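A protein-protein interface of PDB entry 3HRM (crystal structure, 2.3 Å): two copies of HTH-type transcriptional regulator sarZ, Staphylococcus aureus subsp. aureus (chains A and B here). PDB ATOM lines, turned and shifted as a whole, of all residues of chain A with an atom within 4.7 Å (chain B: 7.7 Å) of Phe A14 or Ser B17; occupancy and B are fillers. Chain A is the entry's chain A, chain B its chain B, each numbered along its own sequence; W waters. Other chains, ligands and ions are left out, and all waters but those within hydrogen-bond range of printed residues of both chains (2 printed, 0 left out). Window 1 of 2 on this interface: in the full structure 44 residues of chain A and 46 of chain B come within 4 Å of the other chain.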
ATOM      1  N   LEU A  10     -20.349   5.808 -15.151  1.00  0.00           N
ATOM      2  CA  LEU A  10     -20.085   5.548 -16.558  1.00  0.00           C
ATOM      3  C   LEU A  10     -20.763   4.238 -16.922  1.00  0.00           C
ATOM      4  O   LEU A  10     -21.445   4.123 -17.949  1.00  0.00           O
ATOM      5  CB  LEU A  10     -18.583   5.437 -16.814  1.00  0.00           C
ATOM      6  CG  LEU A  10     -17.798   6.741 -16.693  1.00  0.00           C
ATOM      7  CD1 LEU A  10     -16.326   6.462 -16.828  1.00  0.00           C
ATOM      8  CD2 LEU A  10     -18.255   7.713 -17.754  1.00  0.00           C
ATOM      9  N   CSO A  11     -20.572   3.251 -16.061  1.00  0.00           N
ATOM     10  CA  CSO A  11     -21.162   1.943 -16.270  1.00  0.00           C
ATOM     11  CB  CSO A  11     -20.944   1.065 -15.034  1.00  0.00           C
ATOM     12  SG  CSO A  11     -21.836  -0.517 -15.134  1.00  0.00           S
ATOM     13  C   CSO A  11     -22.654   2.084 -16.560  1.00  0.00           C
ATOM     14  O   CSO A  11     -23.137   1.663 -17.604  1.00  0.00           O
ATOM     15  OD  CSO A  11     -21.220  -1.053 -16.420  1.00  0.00           O
ATOM     16  N   PHE A  12     -23.365   2.706 -15.630  1.00  0.00           N
ATOM     17  CA  PHE A  12     -24.805   2.915 -15.742  1.00  0.00           C
ATOM     18  C   PHE A  12     -25.226   3.655 -17.016  1.00  0.00           C
ATOM     19  O   PHE A  12     -26.009   3.152 -17.816  1.00  0.00           O
ATOM     20  CB  PHE A  12     -25.307   3.700 -14.515  1.00  0.00           C
ATOM     21  CG  PHE A  12     -26.798   3.957 -14.520  1.00  0.00           C
ATOM     22  CD1 PHE A  12     -27.697   2.938 -14.193  1.00  0.00           C
ATOM     23  CD2 PHE A  12     -27.301   5.205 -14.880  1.00  0.00           C
ATOM     24  CE1 PHE A  12     -29.077   3.156 -14.226  1.00  0.00           C
ATOM     25  CE2 PHE A  12     -28.680   5.440 -14.919  1.00  0.00           C
ATOM     26  CZ  PHE A  12     -29.572   4.406 -14.589  1.00  0.00           C
ATOM     27  N   LEU A  13     -24.693   4.854 -17.189  1.00  0.00           N
ATOM     28  CA  LEU A  13     -25.020   5.705 -18.326  1.00  0.00           C
ATOM     29  C   LEU A  13     -24.722   5.138 -19.720  1.00  0.00           C
ATOM     30  O   LEU A  13     -25.470   5.378 -20.668  1.00  0.00           O
ATOM     31  CB  LEU A  13     -24.354   7.064 -18.109  1.00  0.00           C
ATOM     32  CG  LEU A  13     -25.022   7.786 -16.916  1.00  0.00           C
ATOM     33  CD1 LEU A  13     -24.175   8.949 -16.423  1.00  0.00           C
ATOM     34  CD2 LEU A  13     -26.409   8.270 -17.348  1.00  0.00           C
ATOM     35  N   PHE A  14     -23.638   4.385 -19.861  1.00  0.00           N
ATOM     36  CA  PHE A  14     -23.338   3.790 -21.157  1.00  0.00           C
ATOM     37  C   PHE A  14     -24.330   2.665 -21.393  1.00  0.00           C
ATOM     38  O   PHE A  14     -24.785   2.444 -22.510  1.00  0.00           O
ATOM     39  CB  PHE A  14     -21.913   3.233 -21.181  1.00  0.00           C
ATOM     40  CG  PHE A  14     -20.901   4.209 -21.674  1.00  0.00           C
ATOM     41  CD1 PHE A  14     -20.970   4.692 -22.971  1.00  0.00           C
ATOM     42  CD2 PHE A  14     -19.864   4.635 -20.850  1.00  0.00           C
ATOM     43  CE1 PHE A  14     -20.019   5.587 -23.454  1.00  0.00           C
ATOM     44  CE2 PHE A  14     -18.902   5.538 -21.323  1.00  0.00           C
ATOM     45  CZ  PHE A  14     -18.982   6.012 -22.625  1.00  0.00           C
ATOM     46  N   TYR A  15     -24.653   1.945 -20.329  1.00  0.00           N
ATOM     47  CA  TYR A  15     -25.610   0.859 -20.437  1.00  0.00           C
ATOM     48  C   TYR A  15     -26.974   1.426 -20.817  1.00  0.00           C
ATOM     49  O   TYR A  15     -27.582   0.985 -21.782  1.00  0.00           O
ATOM     50  CB  TYR A  15     -25.746   0.113 -19.112  1.00  0.00           C
ATOM     51  CG  TYR A  15     -26.796  -0.976 -19.169  1.00  0.00           C
ATOM     52  CD1 TYR A  15     -26.516  -2.220 -19.748  1.00  0.00           C
ATOM     53  CD2 TYR A  15     -28.076  -0.757 -18.659  1.00  0.00           C
ATOM     54  CE1 TYR A  15     -27.490  -3.219 -19.811  1.00  0.00           C
ATOM     55  CE2 TYR A  15     -29.051  -1.738 -18.719  1.00  0.00           C
ATOM     56  CZ  TYR A  15     -28.755  -2.963 -19.289  1.00  0.00           C
ATOM     57  OH  TYR A  15     -29.723  -3.937 -19.307  1.00  0.00           O
ATOM     58  N   VAL A  16     -27.449   2.407 -20.055  1.00  0.00           N
ATOM     59  CA  VAL A  16     -28.749   3.008 -20.335  1.00  0.00           C
ATOM     60  C   VAL A  16     -28.815   3.658 -21.710  1.00  0.00           C
ATOM     61  O   VAL A  16     -29.817   3.526 -22.417  1.00  0.00           O
ATOM     62  CB  VAL A  16     -29.126   4.062 -19.253  1.00  0.00           C
ATOM     63  CG1 VAL A  16     -30.306   4.910 -19.718  1.00  0.00           C
ATOM     64  CG2 VAL A  16     -29.494   3.351 -17.954  1.00  0.00           C
ATOM     65  N   SER A  17     -27.754   4.364 -22.086  1.00  0.00           N
ATOM     66  CA  SER A  17     -27.709   5.043 -23.378  1.00  0.00           C
ATOM     67  C   SER A  17     -27.825   4.086 -24.561  1.00  0.00           C
ATOM     68  O   SER A  17     -28.557   4.362 -25.510  1.00  0.00           O
ATOM     69  CB  SER A  17     -26.420   5.843 -23.502  1.00  0.00           C
ATOM     70  OG  SER A  17     -25.309   5.005 -23.281  1.00  0.00           O
ATOM     71  N   SER A  18     -27.110   2.967 -24.515  1.00  0.00           N
ATOM     72  CA  SER A  18     -27.177   2.010 -25.611  1.00  0.00           C
ATOM     73  C   SER A  18     -28.563   1.379 -25.683  1.00  0.00           C
ATOM     74  O   SER A  18     -29.098   1.203 -26.783  1.00  0.00           O
ATOM     75  CB  SER A  18     -26.098   0.926 -25.479  1.00  0.00           C
ATOM     76  OG  SER A  18     -26.198   0.252 -24.241  1.00  0.00           O
ATOM     77  N   LEU A 132     -16.693  10.945 -26.851  1.00  0.00           N
ATOM     78  CA  LEU A 132     -16.637   9.540 -27.231  1.00  0.00           C
ATOM     79  C   LEU A 132     -15.478   9.214 -28.152  1.00  0.00           C
ATOM     80  O   LEU A 132     -14.911   8.133 -28.082  1.00  0.00           O
ATOM     81  CB  LEU A 132     -17.970   9.115 -27.861  1.00  0.00           C
ATOM     82  CG  LEU A 132     -19.133   9.254 -26.874  1.00  0.00           C
ATOM     83  CD1 LEU A 132     -20.429   8.691 -27.483  1.00  0.00           C
ATOM     84  CD2 LEU A 132     -18.767   8.492 -25.584  1.00  0.00           C
ATOM     85  N   PHE A 135     -12.733   8.809 -25.688  1.00  0.00           N
ATOM     86  CA  PHE A 135     -12.891   7.613 -24.861  1.00  0.00           C
ATOM     87  C   PHE A 135     -12.515   6.333 -25.625  1.00  0.00           C
ATOM     88  O   PHE A 135     -11.880   5.430 -25.092  1.00  0.00           O
ATOM     89  CB  PHE A 135     -14.343   7.543 -24.378  1.00  0.00           C
ATOM     90  CG  PHE A 135     -14.699   6.270 -23.666  1.00  0.00           C
ATOM     91  CD1 PHE A 135     -15.349   5.238 -24.348  1.00  0.00           C
ATOM     92  CD2 PHE A 135     -14.418   6.109 -22.308  1.00  0.00           C
ATOM     93  CE1 PHE A 135     -15.720   4.064 -23.684  1.00  0.00           C
ATOM     94  CE2 PHE A 135     -14.783   4.940 -21.635  1.00  0.00           C
ATOM     95  CZ  PHE A 135     -15.437   3.916 -22.328  1.00  0.00           C
ATOM     96  N   VAL A 136     -12.898   6.291 -26.891  1.00  0.00           N
ATOM     97  CA  VAL A 136     -12.675   5.141 -27.749  1.00  0.00           C
ATOM     98  C   VAL A 136     -11.327   5.104 -28.471  1.00  0.00           C
ATOM     99  O   VAL A 136     -10.788   4.027 -28.724  1.00  0.00           O
ATOM    100  CB  VAL A 136     -13.827   5.066 -28.795  1.00  0.00           C
ATOM    101  CG1 VAL A 136     -13.273   4.942 -30.221  1.00  0.00           C
ATOM    102  CG2 VAL A 136     -14.762   3.922 -28.447  1.00  0.00           C
ATOM    103  N   LEU B  10     -22.670   9.832 -33.923  1.00  0.00           N
ATOM    104  CA  LEU B  10     -23.263   9.380 -32.670  1.00  0.00           C
ATOM    105  C   LEU B  10     -23.555   7.882 -32.783  1.00  0.00           C
ATOM    106  O   LEU B  10     -23.279   7.113 -31.865  1.00  0.00           O
ATOM    107  CB  LEU B  10     -24.568  10.151 -32.386  1.00  0.00           C
ATOM    108  CG  LEU B  10     -24.380  11.584 -31.873  1.00  0.00           C
ATOM    109  CD1 LEU B  10     -25.698  12.348 -31.852  1.00  0.00           C
ATOM    110  CD2 LEU B  10     -23.779  11.518 -30.488  1.00  0.00           C
ATOM    111  N   CSO B  11     -24.118   7.484 -33.918  1.00  0.00           N
ATOM    112  CA  CSO B  11     -24.446   6.085 -34.151  1.00  0.00           C
ATOM    113  CB  CSO B  11     -24.947   5.893 -35.591  1.00  0.00           C
ATOM    114  SG  CSO B  11     -25.329   4.153 -36.013  1.00  0.00           S
ATOM    115  C   CSO B  11     -23.196   5.238 -33.923  1.00  0.00           C
ATOM    116  O   CSO B  11     -23.163   4.338 -33.067  1.00  0.00           O
ATOM    117  OD  CSO B  11     -26.363   3.906 -34.930  1.00  0.00           O
ATOM    118  N   PHE B  12     -22.163   5.552 -34.692  1.00  0.00           N
ATOM    119  CA  PHE B  12     -20.886   4.851 -34.629  1.00  0.00           C
ATOM    120  C   PHE B  12     -20.214   4.882 -33.246  1.00  0.00           C
ATOM    121  O   PHE B  12     -19.858   3.837 -32.695  1.00  0.00           O
ATOM    122  CB  PHE B  12     -19.939   5.457 -35.683  1.00  0.00           C
ATOM    123  CG  PHE B  12     -18.560   4.831 -35.726  1.00  0.00           C
ATOM    124  CD1 PHE B  12     -18.337   3.635 -36.412  1.00  0.00           C
ATOM    125  CD2 PHE B  12     -17.480   5.449 -35.085  1.00  0.00           C
ATOM    126  CE1 PHE B  12     -17.053   3.057 -36.468  1.00  0.00           C
ATOM    127  CE2 PHE B  12     -16.184   4.887 -35.128  1.00  0.00           C
ATOM    128  CZ  PHE B  12     -15.967   3.686 -35.822  1.00  0.00           C
ATOM    129  N   LEU B  13     -20.037   6.078 -32.686  1.00  0.00           N
ATOM    130  CA  LEU B  13     -19.350   6.207 -31.408  1.00  0.00           C
ATOM    131  C   LEU B  13     -20.050   5.548 -30.222  1.00  0.00           C
ATOM    132  O   LEU B  13     -19.389   4.986 -29.357  1.00  0.00           O
ATOM    133  CB  LEU B  13     -19.041   7.681 -31.137  1.00  0.00           C
ATOM    134  CG  LEU B  13     -17.988   8.237 -32.124  1.00  0.00           C
ATOM    135  CD1 LEU B  13     -17.821   9.746 -31.946  1.00  0.00           C
ATOM    136  CD2 LEU B  13     -16.658   7.530 -31.910  1.00  0.00           C
ATOM    137  N   PHE B  14     -21.378   5.587 -30.187  1.00  0.00           N
ATOM    138  CA  PHE B  14     -22.111   4.942 -29.103  1.00  0.00           C
ATOM    139  C   PHE B  14     -21.992   3.423 -29.269  1.00  0.00           C
ATOM    140  O   PHE B  14     -21.808   2.680 -28.303  1.00  0.00           O
ATOM    141  CB  PHE B  14     -23.586   5.372 -29.133  1.00  0.00           C
ATOM    142  CG  PHE B  14     -23.902   6.514 -28.203  1.00  0.00           C
ATOM    143  CD1 PHE B  14     -23.808   6.343 -26.820  1.00  0.00           C
ATOM    144  CD2 PHE B  14     -24.302   7.759 -28.699  1.00  0.00           C
ATOM    145  CE1 PHE B  14     -24.115   7.404 -25.927  1.00  0.00           C
ATOM    146  CE2 PHE B  14     -24.610   8.825 -27.813  1.00  0.00           C
ATOM    147  CZ  PHE B  14     -24.514   8.635 -26.425  1.00  0.00           C
ATOM    148  N   TYR B  15     -22.109   2.963 -30.508  1.00  0.00           N
ATOM    149  CA  TYR B  15     -21.995   1.549 -30.788  1.00  0.00           C
ATOM    150  C   TYR B  15     -20.604   1.063 -30.376  1.00  0.00           C
ATOM    151  O   TYR B  15     -20.468   0.067 -29.665  1.00  0.00           O
ATOM    152  CB  TYR B  15     -22.187   1.278 -32.283  1.00  0.00           C
ATOM    153  CG  TYR B  15     -22.133  -0.187 -32.620  1.00  0.00           C
ATOM    154  CD1 TYR B  15     -23.247  -0.998 -32.447  1.00  0.00           C
ATOM    155  CD2 TYR B  15     -20.955  -0.775 -33.082  1.00  0.00           C
ATOM    156  CE1 TYR B  15     -23.195  -2.353 -32.720  1.00  0.00           C
ATOM    157  CE2 TYR B  15     -20.895  -2.140 -33.363  1.00  0.00           C
ATOM    158  CZ  TYR B  15     -22.022  -2.918 -33.177  1.00  0.00           C
ATOM    159  OH  TYR B  15     -21.988  -4.264 -33.448  1.00  0.00           O
ATOM    160  N   VAL B  16     -19.564   1.762 -30.813  1.00  0.00           N
ATOM    161  CA  VAL B  16     -18.223   1.320 -30.469  1.00  0.00           C
ATOM    162  C   VAL B  16     -17.915   1.390 -28.981  1.00  0.00           C
ATOM    163  O   VAL B  16     -17.369   0.441 -28.416  1.00  0.00           O
ATOM    164  CB  VAL B  16     -17.161   2.101 -31.263  1.00  0.00           C
ATOM    165  CG1 VAL B  16     -15.759   1.740 -30.762  1.00  0.00           C
ATOM    166  CG2 VAL B  16     -17.277   1.743 -32.741  1.00  0.00           C
ATOM    167  N   SER B  17     -18.267   2.507 -28.350  1.00  0.00           N
ATOM    168  CA  SER B  17     -18.030   2.685 -26.918  1.00  0.00           C
ATOM    169  C   SER B  17     -18.645   1.519 -26.171  1.00  0.00           C
ATOM    170  O   SER B  17     -18.011   0.887 -25.325  1.00  0.00           O
ATOM    171  CB  SER B  17     -18.688   3.981 -26.415  1.00  0.00           C
ATOM    172  OG  SER B  17     -18.088   5.125 -26.992  1.00  0.00           O
ATOM    173  N   SER B  18     -19.901   1.253 -26.494  1.00  0.00           N
ATOM    174  CA  SER B  18     -20.642   0.173 -25.866  1.00  0.00           C
ATOM    175  C   SER B  18     -19.970  -1.165 -26.126  1.00  0.00           C
ATOM    176  O   SER B  18     -19.788  -1.971 -25.204  1.00  0.00           O
ATOM    177  CB  SER B  18     -22.072   0.149 -26.404  1.00  0.00           C
ATOM    178  OG  SER B  18     -22.824  -0.897 -25.816  1.00  0.00           O
ATOM    179  N   LYS B  19     -19.586  -1.411 -27.377  1.00  0.00           N
ATOM    180  CA  LYS B  19     -18.942  -2.682 -27.685  1.00  0.00           C
ATOM    181  C   LYS B  19     -17.605  -2.864 -26.982  1.00  0.00           C
ATOM    182  O   LYS B  19     -17.319  -3.942 -26.471  1.00  0.00           O
ATOM    183  CB  LYS B  19     -18.755  -2.843 -29.188  1.00  0.00           C
ATOM    184  CG  LYS B  19     -20.045  -3.099 -29.920  1.00  0.00           C
ATOM    185  CD  LYS B  19     -20.566  -4.484 -29.595  1.00  0.00           C
ATOM    186  CE  LYS B  19     -21.862  -4.752 -30.338  1.00  0.00           C
ATOM    187  NZ  LYS B  19     -22.145  -6.202 -30.397  1.00  0.00           N
ATOM    188  N   GLU B  20     -16.786  -1.820 -26.943  1.00  0.00           N
ATOM    189  CA  GLU B  20     -15.487  -1.949 -26.293  1.00  0.00           C
ATOM    190  C   GLU B  20     -15.632  -2.218 -24.810  1.00  0.00           C
ATOM    191  O   GLU B  20     -14.822  -2.942 -24.224  1.00  0.00           O
ATOM    192  CB  GLU B  20     -14.641  -0.695 -26.513  1.00  0.00           C
ATOM    193  CG  GLU B  20     -14.175  -0.541 -27.944  1.00  0.00           C
ATOM    194  CD  GLU B  20     -13.366   0.720 -28.153  1.00  0.00           C
ATOM    195  OE1 GLU B  20     -13.286   1.533 -27.214  1.00  0.00           O
ATOM    196  OE2 GLU B  20     -12.816   0.908 -29.258  1.00  0.00           O
ATOM    197  N   ILE B  21     -16.665  -1.637 -24.207  1.00  0.00           N
ATOM    198  CA  ILE B  21     -16.926  -1.816 -22.787  1.00  0.00           C
ATOM    199  C   ILE B  21     -17.367  -3.256 -22.515  1.00  0.00           C
ATOM    200  O   ILE B  21     -16.827  -3.905 -21.615  1.00  0.00           O
ATOM    201  CB  ILE B  21     -18.017  -0.826 -22.285  1.00  0.00           C
ATOM    202  CG1 ILE B  21     -17.437   0.590 -22.168  1.00  0.00           C
ATOM    203  CG2 ILE B  21     -18.560  -1.294 -20.958  1.00  0.00           C
ATOM    204  CD1 ILE B  21     -18.480   1.692 -21.949  1.00  0.00           C
ATOM    205  N   ILE B  22     -18.337  -3.747 -23.295  1.00  0.00           N
ATOM    206  CA  ILE B  22     -18.846  -5.112 -23.147  1.00  0.00           C
ATOM    207  C   ILE B  22     -17.693  -6.104 -23.240  1.00  0.00           C
ATOM    208  O   ILE B  22     -17.512  -6.940 -22.362  1.00  0.00           O
ATOM    209  CB  ILE B  22     -19.853  -5.487 -24.264  1.00  0.00           C
ATOM    210  CG1 ILE B  22     -20.977  -4.459 -24.334  1.00  0.00           C
ATOM    211  CG2 ILE B  22     -20.424  -6.877 -24.018  1.00  0.00           C
ATOM    212  CD1 ILE B  22     -21.701  -4.277 -23.067  1.00  0.00           C
ATOM    213  N   LYS B  23     -16.919  -6.000 -24.318  1.00  0.00           N
ATOM    214  CA  LYS B  23     -15.780  -6.882 -24.543  1.00  0.00           C
ATOM    215  C   LYS B  23     -14.962  -7.068 -23.263  1.00  0.00           C
ATOM    216  O   LYS B  23     -14.793  -8.186 -22.777  1.00  0.00           O
ATOM    217  CB  LYS B  23     -14.903  -6.299 -25.656  1.00  0.00           C
ATOM    218  CG  LYS B  23     -13.904  -7.253 -26.297  1.00  0.00           C
ATOM    219  CD  LYS B  23     -13.061  -6.497 -27.327  1.00  0.00           C
ATOM    220  CE  LYS B  23     -11.932  -7.350 -27.920  1.00  0.00           C
ATOM    221  NZ  LYS B  23     -12.377  -8.270 -29.020  1.00  0.00           N
ATOM    222  N   TYR B  36     -22.495  -9.952 -19.175  1.00  0.00           N
ATOM    223  CA  TYR B  36     -22.506  -8.530 -18.876  1.00  0.00           C
ATOM    224  C   TYR B  36     -23.880  -8.130 -18.324  1.00  0.00           C
ATOM    225  O   TYR B  36     -23.974  -7.402 -17.341  1.00  0.00           O
ATOM    226  CB  TYR B  36     -22.158  -7.757 -20.159  1.00  0.00           C
ATOM    227  CG  TYR B  36     -22.465  -6.280 -20.137  1.00  0.00           C
ATOM    228  CD1 TYR B  36     -21.667  -5.385 -19.426  1.00  0.00           C
ATOM    229  CD2 TYR B  36     -23.536  -5.774 -20.874  1.00  0.00           C
ATOM    230  CE1 TYR B  36     -21.924  -4.011 -19.464  1.00  0.00           C
ATOM    231  CE2 TYR B  36     -23.805  -4.421 -20.916  1.00  0.00           C
ATOM    232  CZ  TYR B  36     -22.997  -3.542 -20.221  1.00  0.00           C
ATOM    233  OH  TYR B  36     -23.231  -2.200 -20.351  1.00  0.00           O
ATOM    234  N   PHE B 115     -13.085   0.384 -16.726  1.00  0.00           N
ATOM    235  CA  PHE B 115     -12.930   1.778 -17.098  1.00  0.00           C
ATOM    236  C   PHE B 115     -11.535   2.383 -16.949  1.00  0.00           C
ATOM    237  O   PHE B 115     -11.173   3.267 -17.723  1.00  0.00           O
ATOM    238  CB  PHE B 115     -14.005   2.597 -16.394  1.00  0.00           C
ATOM    239  CG  PHE B 115     -15.381   2.366 -16.977  1.00  0.00           C
ATOM    240  CD1 PHE B 115     -15.747   2.963 -18.189  1.00  0.00           C
ATOM    241  CD2 PHE B 115     -16.283   1.504 -16.358  1.00  0.00           C
ATOM    242  CE1 PHE B 115     -17.005   2.698 -18.777  1.00  0.00           C
ATOM    243  CE2 PHE B 115     -17.531   1.234 -16.933  1.00  0.00           C
ATOM    244  CZ  PHE B 115     -17.893   1.830 -18.140  1.00  0.00           C
ATOM    245  N   PHE B 118      -9.484   2.439 -20.195  1.00  0.00           N
ATOM    246  CA  PHE B 118      -9.673   3.385 -21.288  1.00  0.00           C
ATOM    247  C   PHE B 118      -8.783   4.602 -21.112  1.00  0.00           C
ATOM    248  O   PHE B 118      -8.572   5.366 -22.049  1.00  0.00           O
ATOM    249  CB  PHE B 118     -11.138   3.805 -21.385  1.00  0.00           C
ATOM    250  CG  PHE B 118     -12.032   2.720 -21.899  1.00  0.00           C
ATOM    251  CD1 PHE B 118     -12.654   1.839 -21.023  1.00  0.00           C
ATOM    252  CD2 PHE B 118     -12.244   2.570 -23.265  1.00  0.00           C
ATOM    253  CE1 PHE B 118     -13.474   0.829 -21.494  1.00  0.00           C
ATOM    254  CE2 PHE B 118     -13.062   1.561 -23.744  1.00  0.00           C
ATOM    255  CZ  PHE B 118     -13.678   0.688 -22.847  1.00  0.00           C
ATOM    256  N   ILE B 120      -8.942   7.681 -19.392  1.00  0.00           N
ATOM    257  CA  ILE B 120      -9.386   9.023 -19.625  1.00  0.00           C
ATOM    258  C   ILE B 120      -9.221   9.599 -18.239  1.00  0.00           C
ATOM    259  O   ILE B 120      -9.125   8.839 -17.273  1.00  0.00           O
ATOM    260  CB  ILE B 120     -10.851   9.088 -20.078  1.00  0.00           C
ATOM    261  CG1 ILE B 120     -11.735   8.244 -19.155  1.00  0.00           C
ATOM    262  CG2 ILE B 120     -10.940   8.663 -21.527  1.00  0.00           C
ATOM    263  CD1 ILE B 120     -13.175   8.702 -19.134  1.00  0.00           C
ATOM    264  N   ALA B 125     -14.043  12.041 -17.624  1.00  0.00           N
ATOM    265  CA  ALA B 125     -15.080  11.118 -17.174  1.00  0.00           C
ATOM    266  C   ALA B 125     -16.299  11.889 -16.671  1.00  0.00           C
ATOM    267  O   ALA B 125     -17.430  11.497 -16.921  1.00  0.00           O
ATOM    268  CB  ALA B 125     -14.531  10.200 -16.062  1.00  0.00           C
ATOM    269  N   ILE B 128     -18.157  13.220 -19.620  1.00  0.00           N
ATOM    270  CA  ILE B 128     -18.941  12.171 -20.256  1.00  0.00           C
ATOM    271  C   ILE B 128     -20.215  11.875 -19.465  1.00  0.00           C
ATOM    272  O   ILE B 128     -21.304  11.742 -20.047  1.00  0.00           O
ATOM    273  CB  ILE B 128     -18.104  10.877 -20.417  1.00  0.00           C
ATOM    274  CG1 ILE B 128     -17.040  11.102 -21.501  1.00  0.00           C
ATOM    275  CG2 ILE B 128     -18.999   9.698 -20.792  1.00  0.00           C
ATOM    276  CD1 ILE B 128     -16.039   9.981 -21.651  1.00  0.00           C
ATOM    277  N   ILE B 129     -20.081  11.766 -18.143  1.00  0.00           N
ATOM    278  CA  ILE B 129     -21.230  11.484 -17.287  1.00  0.00           C
ATOM    279  C   ILE B 129     -22.244  12.615 -17.416  1.00  0.00           C
ATOM    280  O   ILE B 129     -23.426  12.375 -17.673  1.00  0.00           O
ATOM    281  CB  ILE B 129     -20.810  11.318 -15.804  1.00  0.00           C
ATOM    282  CG1 ILE B 129     -19.962  10.055 -15.647  1.00  0.00           C
ATOM    283  CG2 ILE B 129     -22.052  11.238 -14.909  1.00  0.00           C
ATOM    284  CD1 ILE B 129     -19.282   9.922 -14.292  1.00  0.00           C
ATOM    285  N   LEU B 132     -23.870  12.443 -20.686  1.00  0.00           N
ATOM    286  CA  LEU B 132     -24.771  11.297 -20.813  1.00  0.00           C
ATOM    287  C   LEU B 132     -26.020  11.409 -19.927  1.00  0.00           C
ATOM    288  O   LEU B 132     -27.073  10.862 -20.274  1.00  0.00           O
ATOM    289  CB  LEU B 132     -24.037   9.980 -20.520  1.00  0.00           C
ATOM    290  CG  LEU B 132     -23.012   9.499 -21.562  1.00  0.00           C
ATOM    291  CD1 LEU B 132     -22.580   8.074 -21.231  1.00  0.00           C
ATOM    292  CD2 LEU B 132     -23.620   9.543 -22.950  1.00  0.00           C
ATOM    293  N   VAL B 136     -29.725  11.031 -21.595  1.00  0.00           N
ATOM    294  CA  VAL B 136     -30.733  10.077 -21.144  1.00  0.00           C
ATOM    295  C   VAL B 136     -32.046  10.708 -20.640  1.00  0.00           C
ATOM    296  O   VAL B 136     -33.024   9.996 -20.395  1.00  0.00           O
ATOM    297  CB  VAL B 136     -30.136   9.161 -20.034  1.00  0.00           C
ATOM    298  CG1 VAL B 136     -31.208   8.273 -19.437  1.00  0.00           C
ATOM    299  CG2 VAL B 136     -29.027   8.297 -20.625  1.00  0.00           C
HETATM  300  O   HOH W   1     -23.583  -0.638 -23.063  1.00  0.00           O
HETATM  301  O   HOH W   2     -21.929  -0.425 -18.941  1.00  0.00           O
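O of Tyr A15 sits at hydrogen-bond distance from OG of Ser A18, at 2.9 Å. The backbone carbonyl oxygen of Leu A13 lies within hydrogen-bond range of the side-chain hydroxyl of Ser A17, at 2.6 Å. OG of Ser A18 lies within hydrogen-bond range of O of Phe A14 (3.1 Å). The backbone carbonyl oxygen (O) of Leu B13 is in hydrogen-bond range of the side-chain hydroxyl (OG) of Ser B17, 2.7 Å away. The side-chain hydroxyl of Ser A17 is in hydrogen-bond range of the backbone carbonyl oxygen of Phe A14.
CSO A11 touches Phe B115 (N to CZ, 3.7 Å). CB of Leu A13 touches CD1 of Leu B132, 3.7 Å away. CD1 of Tyr A15 touches OH of Tyr B36, at 3.3 Å. Val A16 touches Val B136 (CG1 to CG1, 3.5 Å). CB of Ser A17 touches CE1 of Phe B14, at 3.7 Å. Leu A132 touches Ser B17 (CD2 to OG, 3.7 Å). Phe A135 touches Ser B17 (CD1 to OG, 3.8 Å). Phe B118 touches Phe A135 (CD2 to O, 3.4 Å). Ser B17 touches Val A136. Glu B20 touches Val A136.
Phe A14 touches just these residues of chain B: Ser B17 and Ile B21. Phe B12 touches none of the printed residues of chain A. Ser B17 touches just these residues of chain A: Phe A14, Leu A132, Phe A135 and Val A136. Ile B22 touches none of the printed residues of chain A. Printed residues of chain A within 4 Å of Phe B118: Phe A135 (3.4 Å). Printed residues of chain A within 4 Å of Val B136: Val A16 (3.5 Å). The nearest printed residue of chain B that does not touch Ser A17 is Val B136 (4.4 Å).
Hydrophobic or aromatic side chains of chain B that line the printed part of chain A: Leu B13, Phe B14, Val B16, Ile B21, Tyr B36, Phe B115, Phe B118, Ile B128, Ile B129, Leu B132 and Val B136. Of the 12 printed residues of chain A, 11 touch a printed residue of chain B. Among the printed residues, 21 pairs touch across the chains. Among the printed residues, no Asp or Glu carboxylate lies within 4 Å of a Lys or Arg side-chain nitrogen of the other chain.
Leu A13 touches Leu B132, and with the chains exchanged Leu A132 touches Leu B13. Phe A14 touches Ser B17, and with the chains exchanged Ser A17 touches Phe B14. Val A16 touches Val B136, and with the chains exchanged Val A136 touches Val B16. Val A136 touches Ser B17, but with the chains exchanged Ser A17 does not touch Val B136 (4.4 Å). Positions printed for both chains: 10, 11, 12, 13, 14, 15, 16, 17, 18, 132 and 136. Of the 21 pairs that touch across the chains among the printed residues, 7 have their exchanged pair printed and touching as well.
Water W2 lies within hydrogen-bond range of the side-chain hydroxyl of Tyr B36 (2.6 Å) and OD of CSO A11 (2.7 Å). Water W1 lies within hydrogen-bond range of OG of Ser B18 (2.9 Å), OG of Ser A18 (3.0 Å), OH of Tyr B36 (3.1 Å) and O of Phe A14 (3.4 Å).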
